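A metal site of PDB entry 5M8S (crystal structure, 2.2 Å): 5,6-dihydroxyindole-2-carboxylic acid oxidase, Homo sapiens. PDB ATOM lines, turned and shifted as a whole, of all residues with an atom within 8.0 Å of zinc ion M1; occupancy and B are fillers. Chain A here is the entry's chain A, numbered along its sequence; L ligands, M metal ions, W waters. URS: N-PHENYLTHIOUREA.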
ATOM      1  N   HIS A 168     -22.320   6.059  22.813  1.00  0.00           N
ATOM      2  CA  HIS A 168     -23.042   5.077  22.009  1.00  0.00           C
ATOM      3  C   HIS A 168     -24.472   5.543  21.784  1.00  0.00           C
ATOM      4  O   HIS A 168     -24.979   5.517  20.650  1.00  0.00           O
ATOM      5  CB  HIS A 168     -23.023   3.720  22.717  1.00  0.00           C
ATOM      6  CG  HIS A 168     -23.383   2.535  21.858  1.00  0.00           C
ATOM      7  ND1 HIS A 168     -24.683   2.051  21.749  1.00  0.00           N
ATOM      8  CD2 HIS A 168     -22.613   1.711  21.114  1.00  0.00           C
ATOM      9  CE1 HIS A 168     -24.674   0.980  20.970  1.00  0.00           C
ATOM     10  NE2 HIS A 168     -23.433   0.749  20.575  1.00  0.00           N
ATOM     11  N   SER A 190     -23.148   4.332  14.005  1.00  0.00           N
ATOM     12  CA  SER A 190     -22.233   3.282  14.472  1.00  0.00           C
ATOM     13  C   SER A 190     -22.699   1.871  14.168  1.00  0.00           C
ATOM     14  O   SER A 190     -21.996   0.911  14.538  1.00  0.00           O
ATOM     15  CB  SER A 190     -22.018   3.419  15.991  1.00  0.00           C
ATOM     16  OG  SER A 190     -23.264   3.455  16.658  1.00  0.00           O
ATOM     17  N   HIS A 191     -23.853   1.688  13.518  1.00  0.00           N
ATOM     18  CA  HIS A 191     -24.366   0.370  13.174  1.00  0.00           C
ATOM     19  C   HIS A 191     -24.939   0.414  11.777  1.00  0.00           C
ATOM     20  O   HIS A 191     -25.140   1.490  11.199  1.00  0.00           O
ATOM     21  CB  HIS A 191     -25.455  -0.097  14.139  1.00  0.00           C
ATOM     22  CG  HIS A 191     -25.054   0.000  15.566  1.00  0.00           C
ATOM     23  ND1 HIS A 191     -25.088   1.184  16.278  1.00  0.00           N
ATOM     24  CD2 HIS A 191     -24.520  -0.922  16.410  1.00  0.00           C
ATOM     25  CE1 HIS A 191     -24.657   0.972  17.509  1.00  0.00           C
ATOM     26  NE2 HIS A 191     -24.315  -0.298  17.612  1.00  0.00           N
ATOM     27  N   PHE A 196     -19.367   0.092  11.592  1.00  0.00           N
ATOM     28  CA  PHE A 196     -19.748  -0.652  12.800  1.00  0.00           C
ATOM     29  C   PHE A 196     -18.508  -1.163  13.540  1.00  0.00           C
ATOM     30  O   PHE A 196     -18.392  -0.979  14.757  1.00  0.00           O
ATOM     31  CB  PHE A 196     -20.682  -1.810  12.426  1.00  0.00           C
ATOM     32  CG  PHE A 196     -20.843  -2.841  13.505  1.00  0.00           C
ATOM     33  CD1 PHE A 196     -21.602  -2.562  14.630  1.00  0.00           C
ATOM     34  CD2 PHE A 196     -20.236  -4.090  13.401  1.00  0.00           C
ATOM     35  CE1 PHE A 196     -21.770  -3.521  15.648  1.00  0.00           C
ATOM     36  CE2 PHE A 196     -20.391  -5.052  14.412  1.00  0.00           C
ATOM     37  CZ  PHE A 196     -21.166  -4.762  15.534  1.00  0.00           C
ATOM     38  N   HIS A 200     -16.849   0.697  17.119  1.00  0.00           N
ATOM     39  CA  HIS A 200     -16.818  -0.018  18.398  1.00  0.00           C
ATOM     40  C   HIS A 200     -15.400  -0.316  18.836  1.00  0.00           C
ATOM     41  O   HIS A 200     -15.125  -0.390  20.032  1.00  0.00           O
ATOM     42  CB  HIS A 200     -17.656  -1.285  18.302  1.00  0.00           C
ATOM     43  CG  HIS A 200     -19.123  -1.014  18.236  1.00  0.00           C
ATOM     44  ND1 HIS A 200     -19.745  -0.602  17.081  1.00  0.00           N
ATOM     45  CD2 HIS A 200     -20.083  -1.074  19.184  1.00  0.00           C
ATOM     46  CE1 HIS A 200     -21.032  -0.408  17.315  1.00  0.00           C
ATOM     47  NE2 HIS A 200     -21.265  -0.691  18.585  1.00  0.00           N
ATOM     48  N   HIS A 203     -14.432   2.882  20.542  1.00  0.00           N
ATOM     49  CA  HIS A 203     -15.244   2.864  21.757  1.00  0.00           C
ATOM     50  C   HIS A 203     -14.547   2.055  22.867  1.00  0.00           C
ATOM     51  O   HIS A 203     -14.376   2.553  23.990  1.00  0.00           O
ATOM     52  CB  HIS A 203     -16.617   2.293  21.405  1.00  0.00           C
ATOM     53  CG  HIS A 203     -17.700   2.544  22.425  1.00  0.00           C
ATOM     54  ND1 HIS A 203     -18.680   1.620  22.703  1.00  0.00           N
ATOM     55  CD2 HIS A 203     -17.993   3.633  23.173  1.00  0.00           C
ATOM     56  CE1 HIS A 203     -19.514   2.109  23.600  1.00  0.00           C
ATOM     57  NE2 HIS A 203     -19.118   3.326  23.913  1.00  0.00           N
ATOM     58  N   GLU A 336     -21.700  -8.459  12.137  1.00  0.00           N
ATOM     59  CA  GLU A 336     -22.682  -7.640  12.846  1.00  0.00           C
ATOM     60  C   GLU A 336     -23.949  -8.448  13.128  1.00  0.00           C
ATOM     61  O   GLU A 336     -24.560  -8.319  14.196  1.00  0.00           O
ATOM     62  CB  GLU A 336     -23.019  -6.367  12.050  1.00  0.00           C
ATOM     63  CG  GLU A 336     -23.986  -5.421  12.815  1.00  0.00           C
ATOM     64  CD  GLU A 336     -24.118  -4.010  12.197  1.00  0.00           C
ATOM     65  OE1 GLU A 336     -23.576  -3.783  11.091  1.00  0.00           O
ATOM     66  OE2 GLU A 336     -24.774  -3.133  12.809  1.00  0.00           O
ATOM     67  N   HIS A 353     -23.076 -11.086  16.470  1.00  0.00           N
ATOM     68  CA  HIS A 353     -23.181  -9.931  17.360  1.00  0.00           C
ATOM     69  C   HIS A 353     -24.624  -9.561  17.657  1.00  0.00           C
ATOM     70  O   HIS A 353     -25.004  -9.359  18.821  1.00  0.00           O
ATOM     71  CB  HIS A 353     -22.427  -8.750  16.751  1.00  0.00           C
ATOM     72  CG  HIS A 353     -22.889  -7.402  17.237  1.00  0.00           C
ATOM     73  ND1 HIS A 353     -23.871  -6.678  16.600  1.00  0.00           N
ATOM     74  CD2 HIS A 353     -22.439  -6.623  18.248  1.00  0.00           C
ATOM     75  CE1 HIS A 353     -24.045  -5.528  17.221  1.00  0.00           C
ATOM     76  NE2 HIS A 353     -23.192  -5.477  18.232  1.00  0.00           N
ATOM     77  N   ASN A 354     -25.461  -9.465  16.613  1.00  0.00           N
ATOM     78  CA  ASN A 354     -26.853  -9.099  16.854  1.00  0.00           C
ATOM     79  C   ASN A 354     -27.549 -10.156  17.722  1.00  0.00           C
ATOM     80  O   ASN A 354     -28.311  -9.808  18.631  1.00  0.00           O
ATOM     81  CB  ASN A 354     -27.602  -8.882  15.543  1.00  0.00           C
ATOM     82  CG  ASN A 354     -27.301  -7.518  14.895  1.00  0.00           C
ATOM     83  OD1 ASN A 354     -26.688  -6.636  15.505  1.00  0.00           O
ATOM     84  ND2 ASN A 354     -27.757  -7.321  13.668  1.00  0.00           N
ATOM     85  N   ALA A 356     -26.124 -12.251  19.936  1.00  0.00           N
ATOM     86  CA  ALA A 356     -25.644 -12.188  21.310  1.00  0.00           C
ATOM     87  C   ALA A 356     -26.351 -11.082  22.076  1.00  0.00           C
ATOM     88  O   ALA A 356     -26.734 -11.263  23.239  1.00  0.00           O
ATOM     89  CB  ALA A 356     -24.125 -12.003  21.346  1.00  0.00           C
ATOM     90  N   HIS A 357     -26.582  -9.937  21.423  1.00  0.00           N
ATOM     91  CA  HIS A 357     -27.336  -8.864  22.041  1.00  0.00           C
ATOM     92  C   HIS A 357     -28.753  -9.305  22.376  1.00  0.00           C
ATOM     93  O   HIS A 357     -29.223  -9.130  23.516  1.00  0.00           O
ATOM     94  CB  HIS A 357     -27.383  -7.641  21.123  1.00  0.00           C
ATOM     95  CG  HIS A 357     -26.250  -6.670  21.297  1.00  0.00           C
ATOM     96  ND1 HIS A 357     -26.124  -5.875  22.410  1.00  0.00           N
ATOM     97  CD2 HIS A 357     -25.265  -6.296  20.456  1.00  0.00           C
ATOM     98  CE1 HIS A 357     -25.081  -5.076  22.265  1.00  0.00           C
ATOM     99  NE2 HIS A 357     -24.539  -5.321  21.091  1.00  0.00           N
ATOM    100  N   GLY A 364     -29.269  -4.956  27.838  1.00  0.00           N
ATOM    101  CA  GLY A 364     -28.162  -5.190  26.911  1.00  0.00           C
ATOM    102  C   GLY A 364     -28.587  -5.537  25.498  1.00  0.00           C
ATOM    103  O   GLY A 364     -27.726  -5.638  24.615  1.00  0.00           O
ATOM    104  N   SER A 370     -27.993  -0.564  25.311  1.00  0.00           N
ATOM    105  CA  SER A 370     -27.214  -1.784  25.494  1.00  0.00           C
ATOM    106  C   SER A 370     -25.920  -1.618  26.289  1.00  0.00           C
ATOM    107  O   SER A 370     -25.654  -2.487  27.135  1.00  0.00           O
ATOM    108  CB  SER A 370     -26.975  -2.439  24.131  1.00  0.00           C
ATOM    109  OG  SER A 370     -26.344  -1.569  23.182  1.00  0.00           O
ATOM    110  N   PRO A 371     -25.120  -0.542  26.148  1.00  0.00           N
ATOM    111  CA  PRO A 371     -23.891  -0.457  26.960  1.00  0.00           C
ATOM    112  C   PRO A 371     -24.151  -0.331  28.451  1.00  0.00           C
ATOM    113  O   PRO A 371     -23.206  -0.499  29.239  1.00  0.00           O
ATOM    114  CB  PRO A 371     -23.196   0.800  26.443  1.00  0.00           C
ATOM    115  CG  PRO A 371     -23.831   1.101  25.131  1.00  0.00           C
ATOM    116  CD  PRO A 371     -25.240   0.631  25.266  1.00  0.00           C
ATOM    117  N   PHE A 376     -21.964  -5.774  27.579  1.00  0.00           N
ATOM    118  CA  PHE A 376     -21.654  -5.090  26.321  1.00  0.00           C
ATOM    119  C   PHE A 376     -20.142  -5.015  26.096  1.00  0.00           C
ATOM    120  O   PHE A 376     -19.677  -5.256  24.977  1.00  0.00           O
ATOM    121  CB  PHE A 376     -22.266  -3.674  26.340  1.00  0.00           C
ATOM    122  CG  PHE A 376     -21.983  -2.850  25.096  1.00  0.00           C
ATOM    123  CD1 PHE A 376     -20.773  -2.196  24.930  1.00  0.00           C
ATOM    124  CD2 PHE A 376     -22.972  -2.666  24.144  1.00  0.00           C
ATOM    125  CE1 PHE A 376     -20.519  -1.432  23.815  1.00  0.00           C
ATOM    126  CE2 PHE A 376     -22.738  -1.877  23.028  1.00  0.00           C
ATOM    127  CZ  PHE A 376     -21.501  -1.274  22.858  1.00  0.00           C
ATOM    128  N   LEU A 379     -18.880  -8.484  25.144  1.00  0.00           N
ATOM    129  CA  LEU A 379     -19.453  -8.831  23.853  1.00  0.00           C
ATOM    130  C   LEU A 379     -18.695  -8.149  22.724  1.00  0.00           C
ATOM    131  O   LEU A 379     -18.440  -8.749  21.679  1.00  0.00           O
ATOM    132  CB  LEU A 379     -20.934  -8.435  23.850  1.00  0.00           C
ATOM    133  CG  LEU A 379     -21.878  -8.843  22.715  1.00  0.00           C
ATOM    134  CD1 LEU A 379     -23.315  -8.728  23.186  1.00  0.00           C
ATOM    135  CD2 LEU A 379     -21.681  -7.956  21.447  1.00  0.00           C
ATOM    136  N   HIS A 380     -18.272  -6.901  22.931  1.00  0.00           N
ATOM    137  CA  HIS A 380     -17.636  -6.184  21.830  1.00  0.00           C
ATOM    138  C   HIS A 380     -16.119  -6.346  21.772  1.00  0.00           C
ATOM    139  O   HIS A 380     -15.551  -6.162  20.689  1.00  0.00           O
ATOM    140  CB  HIS A 380     -18.000  -4.696  21.834  1.00  0.00           C
ATOM    141  CG  HIS A 380     -19.247  -4.413  21.065  1.00  0.00           C
ATOM    142  ND1 HIS A 380     -19.274  -4.402  19.682  1.00  0.00           N
ATOM    143  CD2 HIS A 380     -20.519  -4.238  21.469  1.00  0.00           C
ATOM    144  CE1 HIS A 380     -20.513  -4.175  19.281  1.00  0.00           C
ATOM    145  NE2 HIS A 380     -21.280  -4.071  20.338  1.00  0.00           N
ATOM    146  N   THR A 383     -16.212  -9.385  19.552  1.00  0.00           N
ATOM    147  CA  THR A 383     -16.507  -8.916  18.203  1.00  0.00           C
ATOM    148  C   THR A 383     -15.280  -8.249  17.594  1.00  0.00           C
ATOM    149  O   THR A 383     -14.992  -8.411  16.406  1.00  0.00           O
ATOM    150  CB  THR A 383     -17.671  -7.940  18.244  1.00  0.00           C
ATOM    151  OG1 THR A 383     -18.799  -8.553  18.868  1.00  0.00           O
ATOM    152  CG2 THR A 383     -18.066  -7.496  16.817  1.00  0.00           C
HETATM  153  N1  URS L   1     -29.062  -4.718  18.545  1.00  0.00           N
HETATM  154  N2  URS L   1     -30.980  -5.092  19.890  1.00  0.00           N
HETATM  155  C1  URS L   1     -30.742  -4.823  15.140  1.00  0.00           C
HETATM  156  C2  URS L   1     -30.042  -4.337  16.397  1.00  0.00           C
HETATM  157  C3  URS L   1     -29.735  -5.181  17.348  1.00  0.00           C
HETATM  158  C4  URS L   1     -30.097  -6.645  17.215  1.00  0.00           C
HETATM  159  C5  URS L   1     -30.710  -7.082  16.145  1.00  0.00           C
HETATM  160  C6  URS L   1     -31.049  -6.099  15.035  1.00  0.00           C
HETATM  161  C7  URS L   1     -29.770  -4.712  19.815  1.00  0.00           C
HETATM  162  S1  URS L   1     -28.989  -4.205  21.112  1.00  0.00           S
HETATM  163 ZN    ZN M   1     -23.232  -4.273  19.934  1.00  0.00          ZN
HETATM  164 ZN    ZN M   2     -23.214  -0.777  19.298  1.00  0.00          ZN
HETATM  165  O   HOH W   1     -24.153  -2.444  19.911  1.00  0.00           O
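A ring nitrogen (ND1) of His 357 sits close to a sulfur (S1) of the ligand (3.6 Å).
A ring nitrogen (ND1) of His 357 lies within hydrogen-bond range of the backbone carbonyl oxygen (O) of Gly 364, 2.7 Å away.
ND1 of His 353 is in hydrogen-bond range of OD1 of Asn 354, at 3.0 Å.
A ring nitrogen (ND1) of His 353 lies within hydrogen-bond range of the backbone carbonyl oxygen (O) of Glu 336, 3.0 Å away.
Merely in contact with zinc ion M1: Phe 376 (3.9 Å).
Within 4 Å of zinc ion M1: His 353, His 357, Phe 376 and His 380.
The nearest printed residue that does not touch zinc ion M1 is Leu 379 (4.3 Å).
NE2 of His 380 is bound to zinc ion M1 (2.0 Å).
NE2 of His 357 binds zinc ion M1 (2.0 Å).
Water W1 binds zinc ion M1 (2.0 Å).
NE2 of His 353 binds zinc ion M1.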
